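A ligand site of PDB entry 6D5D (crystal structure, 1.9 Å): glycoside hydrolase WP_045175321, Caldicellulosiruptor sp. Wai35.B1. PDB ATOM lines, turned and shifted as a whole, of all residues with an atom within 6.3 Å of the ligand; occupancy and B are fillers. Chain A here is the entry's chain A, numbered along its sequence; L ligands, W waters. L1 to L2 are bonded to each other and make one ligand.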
ATOM      1  N   HIS A  47     -21.467  17.210  -4.683  1.00  0.00           N
ATOM      2  CA  HIS A  47     -22.479  16.353  -5.226  1.00  0.00           C
ATOM      3  C   HIS A  47     -23.689  17.142  -5.756  1.00  0.00           C
ATOM      4  O   HIS A  47     -24.224  16.849  -6.844  1.00  0.00           O
ATOM      5  CB  HIS A  47     -22.971  15.362  -4.182  1.00  0.00           C
ATOM      6  CG  HIS A  47     -24.044  14.474  -4.700  1.00  0.00           C
ATOM      7  ND1 HIS A  47     -23.820  13.455  -5.602  1.00  0.00           N
ATOM      8  CD2 HIS A  47     -25.369  14.457  -4.437  1.00  0.00           C
ATOM      9  CE1 HIS A  47     -24.961  12.840  -5.872  1.00  0.00           C
ATOM     10  NE2 HIS A  47     -25.915  13.414  -5.146  1.00  0.00           N
ATOM     11  N   ILE A  53     -29.700  15.939   1.120  1.00  0.00           N
ATOM     12  CA  ILE A  53     -29.907  14.886   0.114  1.00  0.00           C
ATOM     13  C   ILE A  53     -29.163  13.620   0.563  1.00  0.00           C
ATOM     14  O   ILE A  53     -28.159  13.696   1.212  1.00  0.00           O
ATOM     15  CB  ILE A  53     -29.362  15.319  -1.276  1.00  0.00           C
ATOM     16  CG1 ILE A  53     -29.704  14.340  -2.370  1.00  0.00           C
ATOM     17  CG2 ILE A  53     -27.895  15.793  -1.212  1.00  0.00           C
ATOM     18  CD1 ILE A  53     -29.425  14.892  -3.770  1.00  0.00           C
ATOM     19  N   GLU A  55     -28.563   9.556  -1.035  1.00  0.00           N
ATOM     20  CA  GLU A  55     -28.802   8.567  -2.087  1.00  0.00           C
ATOM     21  C   GLU A  55     -27.638   7.652  -2.441  1.00  0.00           C
ATOM     22  O   GLU A  55     -27.846   6.472  -2.811  1.00  0.00           O
ATOM     23  CB  GLU A  55     -29.331   9.244  -3.356  1.00  0.00           C
ATOM     24  CG  GLU A  55     -28.500  10.406  -3.826  1.00  0.00           C
ATOM     25  CD  GLU A  55     -29.280  11.326  -4.799  1.00  0.00           C
ATOM     26  OE1 GLU A  55     -28.567  11.944  -5.625  1.00  0.00           O
ATOM     27  OE2 GLU A  55     -30.533  11.441  -4.692  1.00  0.00           O
ATOM     28  N   ALA A  56     -26.431   8.197  -2.374  1.00  0.00           N
ATOM     29  CA  ALA A  56     -25.209   7.387  -2.592  1.00  0.00           C
ATOM     30  C   ALA A  56     -24.177   8.034  -1.707  1.00  0.00           C
ATOM     31  O   ALA A  56     -23.756   7.392  -0.697  1.00  0.00           O
ATOM     32  CB  ALA A  56     -24.861   7.302  -4.075  1.00  0.00           C
ATOM     33  N   PRO A  57     -23.864   9.320  -1.946  1.00  0.00           N
ATOM     34  CA  PRO A  57     -23.424  10.121  -0.844  1.00  0.00           C
ATOM     35  C   PRO A  57     -24.662  10.400   0.084  1.00  0.00           C
ATOM     36  O   PRO A  57     -25.808  10.290  -0.397  1.00  0.00           O
ATOM     37  CB  PRO A  57     -22.927  11.404  -1.483  1.00  0.00           C
ATOM     38  CG  PRO A  57     -23.863  11.549  -2.659  1.00  0.00           C
ATOM     39  CD  PRO A  57     -24.133  10.177  -3.123  1.00  0.00           C
ATOM     40  N   THR A  64     -17.823  13.128  -5.081  1.00  0.00           N
ATOM     41  CA  THR A  64     -17.505  11.794  -5.527  1.00  0.00           C
ATOM     42  C   THR A  64     -16.577  11.864  -6.660  1.00  0.00           C
ATOM     43  O   THR A  64     -16.512  12.877  -7.344  1.00  0.00           O
ATOM     44  CB  THR A  64     -18.710  11.047  -6.018  1.00  0.00           C
ATOM     45  OG1 THR A  64     -19.257  11.750  -7.091  1.00  0.00           O
ATOM     46  CG2 THR A  64     -19.736  10.901  -4.935  1.00  0.00           C
ATOM     47  N   GLU A  66     -17.178  10.302  -9.227  1.00  0.00           N
ATOM     48  CA  GLU A  66     -18.187  10.495 -10.276  1.00  0.00           C
ATOM     49  C   GLU A  66     -18.347  11.980 -10.620  1.00  0.00           C
ATOM     50  O   GLU A  66     -18.280  12.297 -11.771  1.00  0.00           O
ATOM     51  CB  GLU A  66     -19.540   9.896  -9.824  1.00  0.00           C
ATOM     52  CG  GLU A  66     -20.783  10.429 -10.480  1.00  0.00           C
ATOM     53  CD  GLU A  66     -22.032   9.876  -9.847  1.00  0.00           C
ATOM     54  OE1 GLU A  66     -22.779  10.664  -9.288  1.00  0.00           O
ATOM     55  OE2 GLU A  66     -22.234   8.628  -9.889  1.00  0.00           O
ATOM     56  N   ASP A 237     -16.225   3.065 -12.544  1.00  0.00           N
ATOM     57  CA  ASP A 237     -17.035   3.729 -13.564  1.00  0.00           C
ATOM     58  C   ASP A 237     -16.662   5.212 -13.779  1.00  0.00           C
ATOM     59  O   ASP A 237     -16.649   5.723 -14.903  1.00  0.00           O
ATOM     60  CB  ASP A 237     -18.546   3.544 -13.244  1.00  0.00           C
ATOM     61  CG  ASP A 237     -19.010   4.191 -11.991  1.00  0.00           C
ATOM     62  OD1 ASP A 237     -18.256   4.327 -10.963  1.00  0.00           O
ATOM     63  OD2 ASP A 237     -20.157   4.607 -11.999  1.00  0.00           O
ATOM     64  N   TRP A 310     -17.016  -3.457  -9.340  1.00  0.00           N
ATOM     65  CA  TRP A 310     -17.549  -2.409  -8.476  1.00  0.00           C
ATOM     66  C   TRP A 310     -16.475  -1.534  -7.804  1.00  0.00           C
ATOM     67  O   TRP A 310     -16.796  -0.423  -7.453  1.00  0.00           O
ATOM     68  CB  TRP A 310     -18.420  -3.018  -7.392  1.00  0.00           C
ATOM     69  CG  TRP A 310     -19.422  -2.072  -6.872  1.00  0.00           C
ATOM     70  CD1 TRP A 310     -19.350  -1.362  -5.736  1.00  0.00           C
ATOM     71  CD2 TRP A 310     -20.693  -1.765  -7.456  1.00  0.00           C
ATOM     72  NE1 TRP A 310     -20.471  -0.618  -5.559  1.00  0.00           N
ATOM     73  CE2 TRP A 310     -21.306  -0.830  -6.622  1.00  0.00           C
ATOM     74  CE3 TRP A 310     -21.305  -2.106  -8.653  1.00  0.00           C
ATOM     75  CZ2 TRP A 310     -22.570  -0.313  -6.879  1.00  0.00           C
ATOM     76  CZ3 TRP A 310     -22.597  -1.583  -8.921  1.00  0.00           C
ATOM     77  CH2 TRP A 310     -23.202  -0.692  -8.050  1.00  0.00           C
ATOM     78  N   PRO A 418     -31.483  -0.258  -2.302  1.00  0.00           N
ATOM     79  CA  PRO A 418     -32.310  -1.052  -3.207  1.00  0.00           C
ATOM     80  C   PRO A 418     -31.406  -1.873  -4.174  1.00  0.00           C
ATOM     81  O   PRO A 418     -30.164  -1.660  -4.197  1.00  0.00           O
ATOM     82  CB  PRO A 418     -33.075   0.041  -3.977  1.00  0.00           C
ATOM     83  CG  PRO A 418     -31.967   1.061  -4.234  1.00  0.00           C
ATOM     84  CD  PRO A 418     -31.266   1.114  -2.852  1.00  0.00           C
ATOM     85  N   TRP A 423     -32.348   0.642 -10.654  1.00  0.00           N
ATOM     86  CA  TRP A 423     -32.220   2.031 -11.055  1.00  0.00           C
ATOM     87  C   TRP A 423     -32.063   2.120 -12.563  1.00  0.00           C
ATOM     88  O   TRP A 423     -31.126   1.623 -13.095  1.00  0.00           O
ATOM     89  CB  TRP A 423     -31.006   2.631 -10.483  1.00  0.00           C
ATOM     90  CG  TRP A 423     -30.873   4.103 -10.741  1.00  0.00           C
ATOM     91  CD1 TRP A 423     -31.793   5.032 -10.489  1.00  0.00           C
ATOM     92  CD2 TRP A 423     -29.709   4.796 -11.218  1.00  0.00           C
ATOM     93  NE1 TRP A 423     -31.308   6.308 -10.748  1.00  0.00           N
ATOM     94  CE2 TRP A 423     -30.028   6.188 -11.223  1.00  0.00           C
ATOM     95  CE3 TRP A 423     -28.434   4.395 -11.625  1.00  0.00           C
ATOM     96  CZ2 TRP A 423     -29.134   7.161 -11.631  1.00  0.00           C
ATOM     97  CZ3 TRP A 423     -27.542   5.374 -12.026  1.00  0.00           C
ATOM     98  CH2 TRP A 423     -27.885   6.733 -12.021  1.00  0.00           C
ATOM     99  N   PHE A 426     -28.656   3.409 -14.873  1.00  0.00           N
ATOM    100  CA  PHE A 426     -27.585   2.630 -15.462  1.00  0.00           C
ATOM    101  C   PHE A 426     -27.803   2.385 -16.951  1.00  0.00           C
ATOM    102  O   PHE A 426     -26.844   2.289 -17.709  1.00  0.00           O
ATOM    103  CB  PHE A 426     -27.277   1.374 -14.697  1.00  0.00           C
ATOM    104  CG  PHE A 426     -26.502   1.608 -13.418  1.00  0.00           C
ATOM    105  CD1 PHE A 426     -25.395   2.434 -13.403  1.00  0.00           C
ATOM    106  CD2 PHE A 426     -26.907   1.016 -12.248  1.00  0.00           C
ATOM    107  CE1 PHE A 426     -24.654   2.637 -12.250  1.00  0.00           C
ATOM    108  CE2 PHE A 426     -26.229   1.243 -11.089  1.00  0.00           C
ATOM    109  CZ  PHE A 426     -25.097   2.060 -11.087  1.00  0.00           C
ATOM    110  N   TRP A 429     -26.616   5.746 -18.619  1.00  0.00           N
ATOM    111  CA  TRP A 429     -25.244   6.055 -18.444  1.00  0.00           C
ATOM    112  C   TRP A 429     -24.347   5.109 -19.195  1.00  0.00           C
ATOM    113  O   TRP A 429     -23.364   5.541 -19.840  1.00  0.00           O
ATOM    114  CB  TRP A 429     -24.897   5.972 -16.950  1.00  0.00           C
ATOM    115  CG  TRP A 429     -25.165   7.178 -16.155  1.00  0.00           C
ATOM    116  CD1 TRP A 429     -25.752   8.394 -16.557  1.00  0.00           C
ATOM    117  CD2 TRP A 429     -24.839   7.327 -14.800  1.00  0.00           C
ATOM    118  NE1 TRP A 429     -25.773   9.246 -15.516  1.00  0.00           N
ATOM    119  CE2 TRP A 429     -25.183   8.612 -14.425  1.00  0.00           C
ATOM    120  CE3 TRP A 429     -24.186   6.494 -13.873  1.00  0.00           C
ATOM    121  CZ2 TRP A 429     -24.933   9.118 -13.165  1.00  0.00           C
ATOM    122  CZ3 TRP A 429     -23.982   6.989 -12.588  1.00  0.00           C
ATOM    123  CH2 TRP A 429     -24.381   8.267 -12.244  1.00  0.00           C
ATOM    124  N   SER A 473     -38.231   4.900 -14.118  1.00  0.00           N
ATOM    125  CA  SER A 473     -37.501   5.253 -12.931  1.00  0.00           C
ATOM    126  C   SER A 473     -36.922   3.993 -12.236  1.00  0.00           C
ATOM    127  O   SER A 473     -35.736   3.911 -12.020  1.00  0.00           O
ATOM    128  CB  SER A 473     -38.419   5.992 -11.978  1.00  0.00           C
ATOM    129  OG  SER A 473     -37.853   5.985 -10.707  1.00  0.00           O
ATOM    130  N   ASP A 504     -36.412  12.112 -13.974  1.00  0.00           N
ATOM    131  CA  ASP A 504     -35.028  12.352 -13.623  1.00  0.00           C
ATOM    132  C   ASP A 504     -34.335  13.018 -14.778  1.00  0.00           C
ATOM    133  O   ASP A 504     -34.147  12.417 -15.867  1.00  0.00           O
ATOM    134  CB  ASP A 504     -34.296  11.018 -13.265  1.00  0.00           C
ATOM    135  CG  ASP A 504     -32.934  11.229 -12.687  1.00  0.00           C
ATOM    136  OD1 ASP A 504     -32.126  11.923 -13.293  1.00  0.00           O
ATOM    137  OD2 ASP A 504     -32.632  10.636 -11.599  1.00  0.00           O
ATOM    138  N   ILE A 507     -30.752  11.662 -15.963  1.00  0.00           N
ATOM    139  CA  ILE A 507     -30.938  10.449 -16.706  1.00  0.00           C
ATOM    140  C   ILE A 507     -31.609  10.691 -18.099  1.00  0.00           C
ATOM    141  O   ILE A 507     -31.240  10.073 -19.097  1.00  0.00           O
ATOM    142  CB  ILE A 507     -31.683   9.399 -15.917  1.00  0.00           C
ATOM    143  CG1 ILE A 507     -30.849   9.022 -14.654  1.00  0.00           C
ATOM    144  CG2 ILE A 507     -31.930   8.200 -16.801  1.00  0.00           C
ATOM    145  CD1 ILE A 507     -29.381   8.619 -14.939  1.00  0.00           C
ATOM    146  N   GLU A 557     -39.216  16.191  -7.174  1.00  0.00           N
ATOM    147  CA  GLU A 557     -39.145  14.770  -6.900  1.00  0.00           C
ATOM    148  C   GLU A 557     -39.553  14.507  -5.448  1.00  0.00           C
ATOM    149  O   GLU A 557     -39.132  15.231  -4.509  1.00  0.00           O
ATOM    150  CB  GLU A 557     -37.752  14.208  -7.203  1.00  0.00           C
ATOM    151  CG  GLU A 557     -36.643  14.422  -6.162  1.00  0.00           C
ATOM    152  CD  GLU A 557     -35.261  13.924  -6.648  1.00  0.00           C
ATOM    153  OE1 GLU A 557     -34.784  14.483  -7.660  1.00  0.00           O
ATOM    154  OE2 GLU A 557     -34.657  13.006  -5.976  1.00  0.00           O
ATOM    155  N   ARG A 559     -39.544  12.311  -2.066  1.00  0.00           N
ATOM    156  CA  ARG A 559     -38.601  11.440  -1.359  1.00  0.00           C
ATOM    157  C   ARG A 559     -39.200  10.918  -0.078  1.00  0.00           C
ATOM    158  O   ARG A 559     -38.799  11.266   0.990  1.00  0.00           O
ATOM    159  CB  ARG A 559     -37.310  12.175  -1.088  1.00  0.00           C
ATOM    160  CG  ARG A 559     -36.572  12.663  -2.350  1.00  0.00           C
ATOM    161  CD  ARG A 559     -36.135  11.533  -3.273  1.00  0.00           C
ATOM    162  NE  ARG A 559     -35.199  10.614  -2.658  1.00  0.00           N
ATOM    163  CZ  ARG A 559     -33.872  10.574  -2.849  1.00  0.00           C
ATOM    164  NH1 ARG A 559     -33.254  11.412  -3.638  1.00  0.00           N
ATOM    165  NH2 ARG A 559     -33.178   9.648  -2.216  1.00  0.00           N
ATOM    166  N   ARG A 624     -28.266  18.439  -8.833  1.00  0.00           N
ATOM    167  CA  ARG A 624     -27.111  17.570  -8.784  1.00  0.00           C
ATOM    168  C   ARG A 624     -26.075  17.982  -9.818  1.00  0.00           C
ATOM    169  O   ARG A 624     -26.403  18.233 -10.962  1.00  0.00           O
ATOM    170  CB  ARG A 624     -27.547  16.117  -9.050  1.00  0.00           C
ATOM    171  CG  ARG A 624     -28.572  15.593  -8.054  1.00  0.00           C
ATOM    172  CD  ARG A 624     -28.999  14.200  -8.417  1.00  0.00           C
ATOM    173  NE  ARG A 624     -29.853  13.520  -7.442  1.00  0.00           N
ATOM    174  CZ  ARG A 624     -31.183  13.656  -7.381  1.00  0.00           C
ATOM    175  NH1 ARG A 624     -31.800  14.522  -8.158  1.00  0.00           N
ATOM    176  NH2 ARG A 624     -31.911  12.968  -6.476  1.00  0.00           N
ATOM    177  N   TRP A 626     -23.797  16.278 -11.394  1.00  0.00           N
ATOM    178  CA  TRP A 626     -23.685  15.352 -12.512  1.00  0.00           C
ATOM    179  C   TRP A 626     -24.864  15.519 -13.458  1.00  0.00           C
ATOM    180  O   TRP A 626     -24.665  15.410 -14.668  1.00  0.00           O
ATOM    181  CB  TRP A 626     -23.519  13.893 -12.031  1.00  0.00           C
ATOM    182  CG  TRP A 626     -24.653  13.236 -11.499  1.00  0.00           C
ATOM    183  CD1 TRP A 626     -24.822  12.951 -10.186  1.00  0.00           C
ATOM    184  CD2 TRP A 626     -25.727  12.581 -12.178  1.00  0.00           C
ATOM    185  NE1 TRP A 626     -25.984  12.281 -10.000  1.00  0.00           N
ATOM    186  CE2 TRP A 626     -26.559  12.030 -11.210  1.00  0.00           C
ATOM    187  CE3 TRP A 626     -26.116  12.456 -13.527  1.00  0.00           C
ATOM    188  CZ2 TRP A 626     -27.740  11.313 -11.524  1.00  0.00           C
ATOM    189  CZ3 TRP A 626     -27.262  11.737 -13.818  1.00  0.00           C
ATOM    190  CH2 TRP A 626     -28.033  11.157 -12.828  1.00  0.00           C
HETATM  191  C1  LIG L   1     -32.265   7.046  -7.136  1.00  0.00           C
HETATM  192  C2  LIG L   1     -30.852   7.338  -6.690  1.00  0.00           C
HETATM  193  C3  LIG L   1     -30.261   8.323  -7.707  1.00  0.00           C
HETATM  194  C4  LIG L   1     -31.131   9.575  -7.964  1.00  0.00           C
HETATM  195  C5  LIG L   1     -30.585  10.448  -9.044  1.00  0.00           C
HETATM  196  C6  LIG L   1     -32.954   8.411  -7.171  1.00  0.00           C
HETATM  197  O1  LIG L   1     -34.275   8.162  -7.410  1.00  0.00           O
HETATM  198  O2  LIG L   1     -32.784   6.057  -6.243  1.00  0.00           O
HETATM  199  O3  LIG L   1     -30.076   6.100  -6.712  1.00  0.00           O
HETATM  200  O4  LIG L   1     -29.053   8.790  -7.199  1.00  0.00           O
HETATM  201  O5  LIG L   1     -32.449   9.171  -8.273  1.00  0.00           O
HETATM  202  O6  LIG L   1     -30.593   9.806 -10.299  1.00  0.00           O
HETATM  203  C1  LG2 L   2     -26.770   9.349  -7.433  1.00  0.00           C
HETATM  204  C2  LG2 L   2     -25.507   8.968  -8.183  1.00  0.00           C
HETATM  205  C3  LG2 L   2     -25.213   7.477  -8.092  1.00  0.00           C
HETATM  206  C4  LG2 L   2     -26.406   6.716  -8.593  1.00  0.00           C
HETATM  207  C5  LG2 L   2     -26.213   5.206  -8.509  1.00  0.00           C
HETATM  208  C6  LG2 L   2     -27.887   8.512  -7.949  1.00  0.00           C
HETATM  209  O1  LG2 L   2     -27.118  10.688  -7.726  1.00  0.00           O
HETATM  210  O2  LG2 L   2     -24.495   9.661  -7.495  1.00  0.00           O
HETATM  211  O3  LG2 L   2     -24.142   7.196  -8.937  1.00  0.00           O
HETATM  212  O4  LG2 L   2     -27.600   7.131  -7.857  1.00  0.00           O
HETATM  213  O5  LG2 L   2     -25.907   4.953  -7.120  1.00  0.00           O
HETATM  214  O   HOH W   1     -27.349   4.918  -5.138  1.00  0.00           O
HETATM  215  O   HOH W   2     -30.519   3.108  -6.989  1.00  0.00           O
HETATM  216  O   HOH W   3     -33.713   8.244 -11.012  1.00  0.00           O
HETATM  217  O   HOH W   4     -35.419  10.814  -7.017  1.00  0.00           O
HETATM  218  O   HOH W   5     -24.692   2.640  -6.457  1.00  0.00           O
HETATM  219  O   HOH W   6     -22.679   5.483  -6.517  1.00  0.00           O
HETATM  220  O   HOH W   7     -22.298   4.690  -9.857  1.00  0.00           O
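OD2 of Asp 504 sits at hydrogen-bond distance from O6 of LIG L1.
The side-chain carboxylate (OE2) of Glu 66 sits at hydrogen-bond distance from an oxygen (O3) of LG2 L2.
OE1 of Glu 55 sits at hydrogen-bond distance from O1 of LG2 L2.
The indole nitrogen (NE1) of Trp 626 lies within hydrogen-bond range of an oxygen (O1) of LG2 L2 (3.0 Å).
OD1 of Asp 504 sits at hydrogen-bond distance from N of Ile 507 (3.0 Å).
The side-chain hydroxyl (OG1) of Thr 64 lies close to the backbone NH (N) of Glu 66 (3.3 Å).
NH2 of Arg 624 lies within salt-bridge range of OE2 of Glu 55 (2.7 Å).
A ring nitrogen (NE2) of His 47 is in hydrogen-bond range of the side-chain carboxylate (OE1) of Glu 55, at 3.1 Å.
The side-chain carboxylate (OE2) of Glu 55 is in salt-bridge range of the guanidinium group (NH1) of Arg 559 (2.9 Å).
The side-chain carboxylate (OE2) of Glu 557 lies within salt-bridge range of the guanidinium group (NH2) of Arg 624.
Merely in contact with the ligand: His 47 (3.6 Å), Ala 56 (3.99 Å), Trp 423 (3.3 Å), Trp 429 (3.5 Å) and Arg 624 (3.5 Å).
Nine residues have an atom within 4 Å of the ligand: His 47, Glu 55, Ala 56, Glu 66, Trp 423, Trp 429, Asp 504, Arg 624 and Trp 626.
Water W1 lies within hydrogen-bond range of O5 of LG2 L2 (2.5 Å) and O of Glu 55 (2.8 Å).
Water W4 lies within hydrogen-bond range of OE2 of Glu 557 (2.5 Å) and O1 of LIG L1 (2.9 Å).
Water W3 lies within hydrogen-bond range of the side-chain carboxylate of Asp 504, the indole nitrogen of Trp 423 and an oxygen (O5) of LIG L1.
Water W7 bridges the side-chain carboxylate (OD2) of Asp 237 and an oxygen (O3) of LG2 L2.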
